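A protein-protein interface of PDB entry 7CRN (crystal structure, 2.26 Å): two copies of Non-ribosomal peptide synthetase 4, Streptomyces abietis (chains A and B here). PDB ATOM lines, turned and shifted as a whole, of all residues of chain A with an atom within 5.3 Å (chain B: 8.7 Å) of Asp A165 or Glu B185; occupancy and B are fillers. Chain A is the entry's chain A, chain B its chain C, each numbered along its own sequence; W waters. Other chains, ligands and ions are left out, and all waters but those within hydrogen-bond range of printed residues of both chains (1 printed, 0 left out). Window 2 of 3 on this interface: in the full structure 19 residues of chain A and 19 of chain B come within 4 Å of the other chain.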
ATOM      1  N   GLN A 142       4.318 -33.093  13.180  1.00  0.00           N
ATOM      2  CA  GLN A 142       3.457 -33.413  14.309  1.00  0.00           C
ATOM      3  C   GLN A 142       4.270 -33.910  15.496  1.00  0.00           C
ATOM      4  O   GLN A 142       3.920 -33.636  16.650  1.00  0.00           O
ATOM      5  CB  GLN A 142       2.417 -34.446  13.881  1.00  0.00           C
ATOM      6  CG  GLN A 142       1.436 -33.897  12.859  1.00  0.00           C
ATOM      7  CD  GLN A 142       0.543 -32.814  13.444  1.00  0.00           C
ATOM      8  OE1 GLN A 142      -0.182 -33.050  14.406  1.00  0.00           O
ATOM      9  NE2 GLN A 142       0.596 -31.619  12.865  1.00  0.00           N
ATOM     10  N   LEU A 145       5.743 -30.869  17.249  1.00  0.00           N
ATOM     11  CA  LEU A 145       4.721 -30.240  18.081  1.00  0.00           C
ATOM     12  C   LEU A 145       4.433 -31.066  19.332  1.00  0.00           C
ATOM     13  O   LEU A 145       4.209 -30.505  20.413  1.00  0.00           O
ATOM     14  CB  LEU A 145       3.440 -30.029  17.275  1.00  0.00           C
ATOM     15  CG  LEU A 145       3.586 -29.098  16.068  1.00  0.00           C
ATOM     16  CD1 LEU A 145       2.280 -29.014  15.280  1.00  0.00           C
ATOM     17  CD2 LEU A 145       4.041 -27.727  16.524  1.00  0.00           C
ATOM     18  N   PRO A 163      -4.614 -34.003  14.930  1.00  0.00           N
ATOM     19  CA  PRO A 163      -3.812 -33.065  14.130  1.00  0.00           C
ATOM     20  C   PRO A 163      -3.483 -31.787  14.897  1.00  0.00           C
ATOM     21  O   PRO A 163      -4.362 -30.946  15.091  1.00  0.00           O
ATOM     22  CB  PRO A 163      -4.712 -32.761  12.929  1.00  0.00           C
ATOM     23  CG  PRO A 163      -6.100 -33.021  13.406  1.00  0.00           C
ATOM     24  CD  PRO A 163      -6.033 -34.018  14.532  1.00  0.00           C
ATOM     25  N   LEU A 164      -2.234 -31.650  15.333  1.00  0.00           N
ATOM     26  CA  LEU A 164      -1.841 -30.482  16.102  1.00  0.00           C
ATOM     27  C   LEU A 164      -1.503 -29.321  15.178  1.00  0.00           C
ATOM     28  O   LEU A 164      -1.153 -29.503  14.008  1.00  0.00           O
ATOM     29  CB  LEU A 164      -0.639 -30.799  16.989  1.00  0.00           C
ATOM     30  CG  LEU A 164      -0.796 -31.987  17.936  1.00  0.00           C
ATOM     31  CD1 LEU A 164       0.521 -32.291  18.633  1.00  0.00           C
ATOM     32  CD2 LEU A 164      -1.897 -31.705  18.951  1.00  0.00           C
ATOM     33  N   ASP A 165      -1.593 -28.109  15.724  1.00  0.00           N
ATOM     34  CA  ASP A 165      -1.228 -26.915  14.976  1.00  0.00           C
ATOM     35  C   ASP A 165      -0.405 -25.990  15.860  1.00  0.00           C
ATOM     36  O   ASP A 165      -0.458 -26.055  17.090  1.00  0.00           O
ATOM     37  CB  ASP A 165      -2.461 -26.188  14.416  1.00  0.00           C
ATOM     38  CG  ASP A 165      -3.298 -25.530  15.493  1.00  0.00           C
ATOM     39  OD1 ASP A 165      -4.125 -26.229  16.116  1.00  0.00           O
ATOM     40  OD2 ASP A 165      -3.135 -24.310  15.707  1.00  0.00           O
ATOM     41  N   TYR A 166       0.367 -25.122  15.200  1.00  0.00           N
ATOM     42  CA  TYR A 166       1.314 -24.263  15.906  1.00  0.00           C
ATOM     43  C   TYR A 166       0.608 -23.323  16.875  1.00  0.00           C
ATOM     44  O   TYR A 166       1.111 -23.068  17.974  1.00  0.00           O
ATOM     45  CB  TYR A 166       2.140 -23.459  14.903  1.00  0.00           C
ATOM     46  CG  TYR A 166       3.344 -24.183  14.337  1.00  0.00           C
ATOM     47  CD1 TYR A 166       4.559 -24.189  15.013  1.00  0.00           C
ATOM     48  CD2 TYR A 166       3.270 -24.849  13.117  1.00  0.00           C
ATOM     49  CE1 TYR A 166       5.670 -24.847  14.493  1.00  0.00           C
ATOM     50  CE2 TYR A 166       4.375 -25.510  12.587  1.00  0.00           C
ATOM     51  CZ  TYR A 166       5.572 -25.503  13.276  1.00  0.00           C
ATOM     52  OH  TYR A 166       6.671 -26.155  12.753  1.00  0.00           O
ATOM     53  N   ALA A 167      -0.548 -22.784  16.478  1.00  0.00           N
ATOM     54  CA  ALA A 167      -1.232 -21.803  17.318  1.00  0.00           C
ATOM     55  C   ALA A 167      -1.678 -22.414  18.642  1.00  0.00           C
ATOM     56  O   ALA A 167      -1.514 -21.801  19.707  1.00  0.00           O
ATOM     57  CB  ALA A 167      -2.425 -21.219  16.566  1.00  0.00           C
ATOM     58  N   MET A 168      -2.212 -23.629  18.580  1.00  0.00           N
ATOM     59  CA  MET A 168      -2.667 -24.326  19.777  1.00  0.00           C
ATOM     60  C   MET A 168      -1.507 -24.600  20.731  1.00  0.00           C
ATOM     61  O   MET A 168      -1.625 -24.399  21.940  1.00  0.00           O
ATOM     62  CB  MET A 168      -3.362 -25.638  19.405  1.00  0.00           C
ATOM     63  CG  MET A 168      -3.989 -26.364  20.584  1.00  0.00           C
ATOM     64  SD  MET A 168      -2.809 -27.402  21.468  1.00  0.00           S
ATOM     65  CE  MET A 168      -3.555 -27.452  23.095  1.00  0.00           C
ATOM     66  N   VAL A 169      -0.385 -25.058  20.182  1.00  0.00           N
ATOM     67  CA  VAL A 169       0.793 -25.356  20.986  1.00  0.00           C
ATOM     68  C   VAL A 169       1.342 -24.085  21.614  1.00  0.00           C
ATOM     69  O   VAL A 169       1.734 -24.075  22.788  1.00  0.00           O
ATOM     70  CB  VAL A 169       1.853 -26.062  20.121  1.00  0.00           C
ATOM     71  CG1 VAL A 169       3.181 -26.114  20.850  1.00  0.00           C
ATOM     72  CG2 VAL A 169       1.378 -27.457  19.744  1.00  0.00           C
ATOM     73  N   ALA A 170       1.373 -22.995  20.849  1.00  0.00           N
ATOM     74  CA  ALA A 170       1.853 -21.728  21.385  1.00  0.00           C
ATOM     75  C   ALA A 170       0.979 -21.253  22.534  1.00  0.00           C
ATOM     76  O   ALA A 170       1.487 -20.734  23.534  1.00  0.00           O
ATOM     77  CB  ALA A 170       1.909 -20.672  20.282  1.00  0.00           C
ATOM     78  N   PRO B  63      -4.750 -32.765   5.831  1.00  0.00           N
ATOM     79  CA  PRO B  63      -3.496 -32.631   6.594  1.00  0.00           C
ATOM     80  C   PRO B  63      -2.981 -33.943   7.167  1.00  0.00           C
ATOM     81  O   PRO B  63      -1.840 -33.978   7.646  1.00  0.00           O
ATOM     82  CB  PRO B  63      -3.869 -31.646   7.712  1.00  0.00           C
ATOM     83  CG  PRO B  63      -5.046 -30.887   7.164  1.00  0.00           C
ATOM     84  CD  PRO B  63      -5.819 -31.916   6.383  1.00  0.00           C
ATOM     85  N   TYR B 166       3.161 -16.290   9.130  1.00  0.00           N
ATOM     86  CA  TYR B 166       2.043 -17.015   8.538  1.00  0.00           C
ATOM     87  C   TYR B 166       0.706 -16.389   8.908  1.00  0.00           C
ATOM     88  O   TYR B 166      -0.200 -16.319   8.073  1.00  0.00           O
ATOM     89  CB  TYR B 166       2.073 -18.478   8.978  1.00  0.00           C
ATOM     90  CG  TYR B 166       2.917 -19.381   8.100  1.00  0.00           C
ATOM     91  CD1 TYR B 166       2.397 -19.948   6.941  1.00  0.00           C
ATOM     92  CD2 TYR B 166       4.233 -19.669   8.438  1.00  0.00           C
ATOM     93  CE1 TYR B 166       3.170 -20.782   6.138  1.00  0.00           C
ATOM     94  CE2 TYR B 166       5.014 -20.495   7.646  1.00  0.00           C
ATOM     95  CZ  TYR B 166       4.479 -21.050   6.501  1.00  0.00           C
ATOM     96  OH  TYR B 166       5.265 -21.871   5.727  1.00  0.00           O
ATOM     97  N   ALA B 167       0.555 -15.947  10.158  1.00  0.00           N
ATOM     98  CA  ALA B 167      -0.733 -15.411  10.593  1.00  0.00           C
ATOM     99  C   ALA B 167      -1.095 -14.144   9.829  1.00  0.00           C
ATOM    100  O   ALA B 167      -2.252 -13.962   9.434  1.00  0.00           O
ATOM    101  CB  ALA B 167      -0.717 -15.145  12.096  1.00  0.00           C
ATOM    102  N   MET B 168      -0.124 -13.254   9.613  1.00  0.00           N
ATOM    103  CA  MET B 168      -0.399 -12.025   8.876  1.00  0.00           C
ATOM    104  C   MET B 168      -0.783 -12.327   7.429  1.00  0.00           C
ATOM    105  O   MET B 168      -1.711 -11.719   6.877  1.00  0.00           O
ATOM    106  CB  MET B 168       0.820 -11.097   8.947  1.00  0.00           C
ATOM    107  CG  MET B 168       0.771  -9.879   8.027  1.00  0.00           C
ATOM    108  SD  MET B 168       1.450 -10.191   6.379  1.00  0.00           S
ATOM    109  CE  MET B 168       1.476  -8.533   5.694  1.00  0.00           C
ATOM    110  N   ALA B 170      -2.096 -15.132   6.318  1.00  0.00           N
ATOM    111  CA  ALA B 170      -3.413 -15.750   6.363  1.00  0.00           C
ATOM    112  C   ALA B 170      -4.500 -14.702   6.541  1.00  0.00           C
ATOM    113  O   ALA B 170      -5.576 -14.813   5.952  1.00  0.00           O
ATOM    114  CB  ALA B 170      -3.476 -16.778   7.490  1.00  0.00           C
ATOM    115  N   ASP B 171      -4.243 -13.687   7.365  1.00  0.00           N
ATOM    116  CA  ASP B 171      -5.240 -12.641   7.562  1.00  0.00           C
ATOM    117  C   ASP B 171      -5.437 -11.831   6.290  1.00  0.00           C
ATOM    118  O   ASP B 171      -6.569 -11.479   5.952  1.00  0.00           O
ATOM    119  CB  ASP B 171      -4.849 -11.725   8.724  1.00  0.00           C
ATOM    120  CG  ASP B 171      -5.181 -12.326  10.078  1.00  0.00           C
ATOM    121  OD1 ASP B 171      -6.088 -13.182  10.151  1.00  0.00           O
ATOM    122  OD2 ASP B 171      -4.537 -11.927  11.071  1.00  0.00           O
ATOM    123  N   ARG B 174      -7.426 -14.216   3.915  1.00  0.00           N
ATOM    124  CA  ARG B 174      -8.828 -14.398   4.264  1.00  0.00           C
ATOM    125  C   ARG B 174      -9.581 -13.114   4.081  1.00  0.00           C
ATOM    126  O   ARG B 174     -10.782 -13.149   3.691  1.00  0.00           O
ATOM    127  CB  ARG B 174      -9.019 -14.823   5.712  1.00  0.00           C
ATOM    128  CG  ARG B 174      -8.451 -16.094   6.199  1.00  0.00           C
ATOM    129  CD  ARG B 174      -8.909 -16.126   7.657  1.00  0.00           C
ATOM    130  NE  ARG B 174      -8.165 -17.107   8.405  1.00  0.00           N
ATOM    131  CZ  ARG B 174      -7.140 -16.806   9.187  1.00  0.00           C
ATOM    132  NH1 ARG B 174      -6.505 -17.785   9.809  1.00  0.00           N
ATOM    133  NH2 ARG B 174      -6.746 -15.540   9.337  1.00  0.00           N
ATOM    134  N   ALA B 181     -11.649 -17.902   3.115  1.00  0.00           N
ATOM    135  CA  ALA B 181     -12.323 -17.567   4.368  1.00  0.00           C
ATOM    136  C   ALA B 181     -12.126 -18.650   5.421  1.00  0.00           C
ATOM    137  O   ALA B 181     -11.750 -18.357   6.561  1.00  0.00           O
ATOM    138  CB  ALA B 181     -13.810 -17.327   4.112  1.00  0.00           C
ATOM    139  N   ASN B 182     -12.372 -19.911   5.061  1.00  0.00           N
ATOM    140  CA  ASN B 182     -12.212 -21.024   6.000  1.00  0.00           C
ATOM    141  C   ASN B 182     -10.790 -21.566   6.021  1.00  0.00           C
ATOM    142  O   ASN B 182     -10.576 -22.779   6.123  1.00  0.00           O
ATOM    143  CB  ASN B 182     -13.209 -22.132   5.676  1.00  0.00           C
ATOM    144  CG  ASN B 182     -14.554 -21.594   5.230  1.00  0.00           C
ATOM    145  OD1 ASN B 182     -14.989 -21.835   4.104  1.00  0.00           O
ATOM    146  ND2 ASN B 182     -15.222 -20.858   6.115  1.00  0.00           N
ATOM    147  N   LEU B 183      -9.797 -20.681   5.937  1.00  0.00           N
ATOM    148  CA  LEU B 183      -8.391 -21.034   6.122  1.00  0.00           C
ATOM    149  C   LEU B 183      -8.044 -20.847   7.598  1.00  0.00           C
ATOM    150  O   LEU B 183      -7.878 -19.718   8.072  1.00  0.00           O
ATOM    151  CB  LEU B 183      -7.515 -20.179   5.212  1.00  0.00           C
ATOM    152  CG  LEU B 183      -6.007 -20.387   5.139  1.00  0.00           C
ATOM    153  CD1 LEU B 183      -5.666 -21.429   4.087  1.00  0.00           C
ATOM    154  CD2 LEU B 183      -5.324 -19.064   4.823  1.00  0.00           C
ATOM    155  N   ASP B 184      -7.945 -21.958   8.331  1.00  0.00           N
ATOM    156  CA  ASP B 184      -7.805 -21.948   9.780  1.00  0.00           C
ATOM    157  C   ASP B 184      -6.364 -22.274  10.194  1.00  0.00           C
ATOM    158  O   ASP B 184      -5.458 -22.411   9.361  1.00  0.00           O
ATOM    159  CB  ASP B 184      -8.811 -22.919  10.410  1.00  0.00           C
ATOM    160  CG  ASP B 184      -8.805 -24.295   9.750  1.00  0.00           C
ATOM    161  OD1 ASP B 184      -7.937 -24.550   8.884  1.00  0.00           O
ATOM    162  OD2 ASP B 184      -9.672 -25.128  10.103  1.00  0.00           O
ATOM    163  N   GLU B 185      -6.147 -22.412  11.504  1.00  0.00           N
ATOM    164  CA  GLU B 185      -4.810 -22.724  12.003  1.00  0.00           C
ATOM    165  C   GLU B 185      -4.375 -24.126  11.594  1.00  0.00           C
ATOM    166  O   GLU B 185      -3.177 -24.373  11.397  1.00  0.00           O
ATOM    167  CB  GLU B 185      -4.774 -22.565  13.520  1.00  0.00           C
ATOM    168  CG  GLU B 185      -4.994 -21.126  13.983  1.00  0.00           C
ATOM    169  CD  GLU B 185      -4.061 -20.132  13.292  1.00  0.00           C
ATOM    170  OE1 GLU B 185      -2.841 -20.400  13.215  1.00  0.00           O
ATOM    171  OE2 GLU B 185      -4.551 -19.077  12.827  1.00  0.00           O
ATOM    172  N   THR B 186      -5.333 -25.046  11.452  1.00  0.00           N
ATOM    173  CA  THR B 186      -5.035 -26.348  10.862  1.00  0.00           C
ATOM    174  C   THR B 186      -4.403 -26.191   9.481  1.00  0.00           C
ATOM    175  O   THR B 186      -3.366 -26.799   9.190  1.00  0.00           O
ATOM    176  CB  THR B 186      -6.310 -27.191  10.781  1.00  0.00           C
ATOM    177  OG1 THR B 186      -6.751 -27.511  12.108  1.00  0.00           O
ATOM    178  CG2 THR B 186      -6.052 -28.487  10.028  1.00  0.00           C
ATOM    179  N   ALA B 187      -4.993 -25.347   8.626  1.00  0.00           N
ATOM    180  CA  ALA B 187      -4.477 -25.182   7.270  1.00  0.00           C
ATOM    181  C   ALA B 187      -3.138 -24.455   7.273  1.00  0.00           C
ATOM    182  O   ALA B 187      -2.256 -24.777   6.472  1.00  0.00           O
ATOM    183  CB  ALA B 187      -5.493 -24.440   6.400  1.00  0.00           C
ATOM    184  N   ILE B 188      -2.969 -23.466   8.153  1.00  0.00           N
ATOM    185  CA  ILE B 188      -1.685 -22.770   8.255  1.00  0.00           C
ATOM    186  C   ILE B 188      -0.573 -23.754   8.613  1.00  0.00           C
ATOM    187  O   ILE B 188       0.502 -23.769   7.991  1.00  0.00           O
ATOM    188  CB  ILE B 188      -1.785 -21.629   9.284  1.00  0.00           C
ATOM    189  CG1 ILE B 188      -2.687 -20.513   8.754  1.00  0.00           C
ATOM    190  CG2 ILE B 188      -0.406 -21.086   9.634  1.00  0.00           C
ATOM    191  CD1 ILE B 188      -3.029 -19.468   9.791  1.00  0.00           C
ATOM    192  N   THR B 189      -0.827 -24.607   9.612  1.00  0.00           N
ATOM    193  CA  THR B 189       0.156 -25.613   9.999  1.00  0.00           C
ATOM    194  C   THR B 189       0.395 -26.620   8.879  1.00  0.00           C
ATOM    195  O   THR B 189       1.529 -27.051   8.662  1.00  0.00           O
ATOM    196  CB  THR B 189      -0.293 -26.313  11.283  1.00  0.00           C
ATOM    197  OG1 THR B 189      -0.225 -25.379  12.364  1.00  0.00           O
ATOM    198  CG2 THR B 189       0.603 -27.494  11.603  1.00  0.00           C
ATOM    199  N   ALA B 190      -0.659 -27.004   8.152  1.00  0.00           N
ATOM    200  CA  ALA B 190      -0.479 -27.895   7.008  1.00  0.00           C
ATOM    201  C   ALA B 190       0.380 -27.245   5.919  1.00  0.00           C
ATOM    202  O   ALA B 190       1.175 -27.924   5.256  1.00  0.00           O
ATOM    203  CB  ALA B 190      -1.844 -28.308   6.454  1.00  0.00           C
ATOM    204  N   LEU B 191       0.232 -25.933   5.718  1.00  0.00           N
ATOM    205  CA  LEU B 191       1.096 -25.219   4.776  1.00  0.00           C
ATOM    206  C   LEU B 191       2.551 -25.286   5.216  1.00  0.00           C
ATOM    207  O   LEU B 191       3.451 -25.522   4.401  1.00  0.00           O
ATOM    208  CB  LEU B 191       0.662 -23.755   4.645  1.00  0.00           C
ATOM    209  CG  LEU B 191      -0.605 -23.403   3.870  1.00  0.00           C
ATOM    210  CD1 LEU B 191      -0.931 -21.923   4.051  1.00  0.00           C
ATOM    211  CD2 LEU B 191      -0.445 -23.749   2.398  1.00  0.00           C
ATOM    212  N   ALA B 192       2.802 -25.036   6.505  1.00  0.00           N
ATOM    213  CA  ALA B 192       4.164 -25.161   7.028  1.00  0.00           C
ATOM    214  C   ALA B 192       4.707 -26.580   6.844  1.00  0.00           C
ATOM    215  O   ALA B 192       5.871 -26.770   6.466  1.00  0.00           O
ATOM    216  CB  ALA B 192       4.193 -24.768   8.504  1.00  0.00           C
HETATM  217  O   HOH W   1      -1.317 -22.874  13.357  1.00  0.00           O
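The side-chain amide oxygen of Gln A142 is in hydrogen-bond range of the backbone NH of Leu A164 (2.7 Å). OD2 of Asp A165 sits at hydrogen-bond distance from N of Ala A167 (3.1 Å). N of Met A168 is in hydrogen-bond range of OD2 of Asp A165, at 3.1 Å. The side-chain carboxylate (OE2) of Glu B185 is in salt-bridge range of the guanidinium group (NH1) of Arg B174 (3.8 Å). OG1 of Thr B189 lies within hydrogen-bond range of O of Glu B185 (3.3 Å).
Of chain B, only Glu B185 and Thr B189 come within 4 Å of Asp A165. Glu B185 touches two residues of chain A. Printed residues of chain A within 4 Å of Thr B189: Leu A164, Asp A165 and Tyr A166. Printed residues of chain B within 4 Å of Tyr A166: Thr B189 (2.9 Å). Ala B187 touches none of the printed residues of chain A. Asn B182 touches none of the printed residues of chain A. The nearest residue of chain B that does not touch Asp A165 is Thr B186 (4.3 Å). The nearest printed residue of chain A that does not touch Glu B185 is Tyr A166 (5.3 Å). The nearest printed residue of chain B that does not touch Ala A167 is Thr B189 (4.9 Å).
Along chain B the printed residues that touch a printed residue of chain A span positions 185 to 189.
Among the printed residues, pairs that only touch across the chains: Leu A164 with Thr B189, Asp A165 with Glu B185, Asp A165 with Thr B189 and Ala A167 with Glu B185.
The backbone NH (N) of Tyr A166 lies within hydrogen-bond range of the side-chain hydroxyl (OG1) of Thr B189 (2.9 Å).
Water W1 lies within hydrogen-bond range of OG1 of Thr B189 (2.9 Å), OE1 of Glu B185 (2.9 Å), N of Ala A167 (3.2 Å), OD2 of Asp A165 (3.3 Å) and N of Tyr A166 (3.4 Å).
Positions printed for both chains: 166, 167, 168 and 170.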
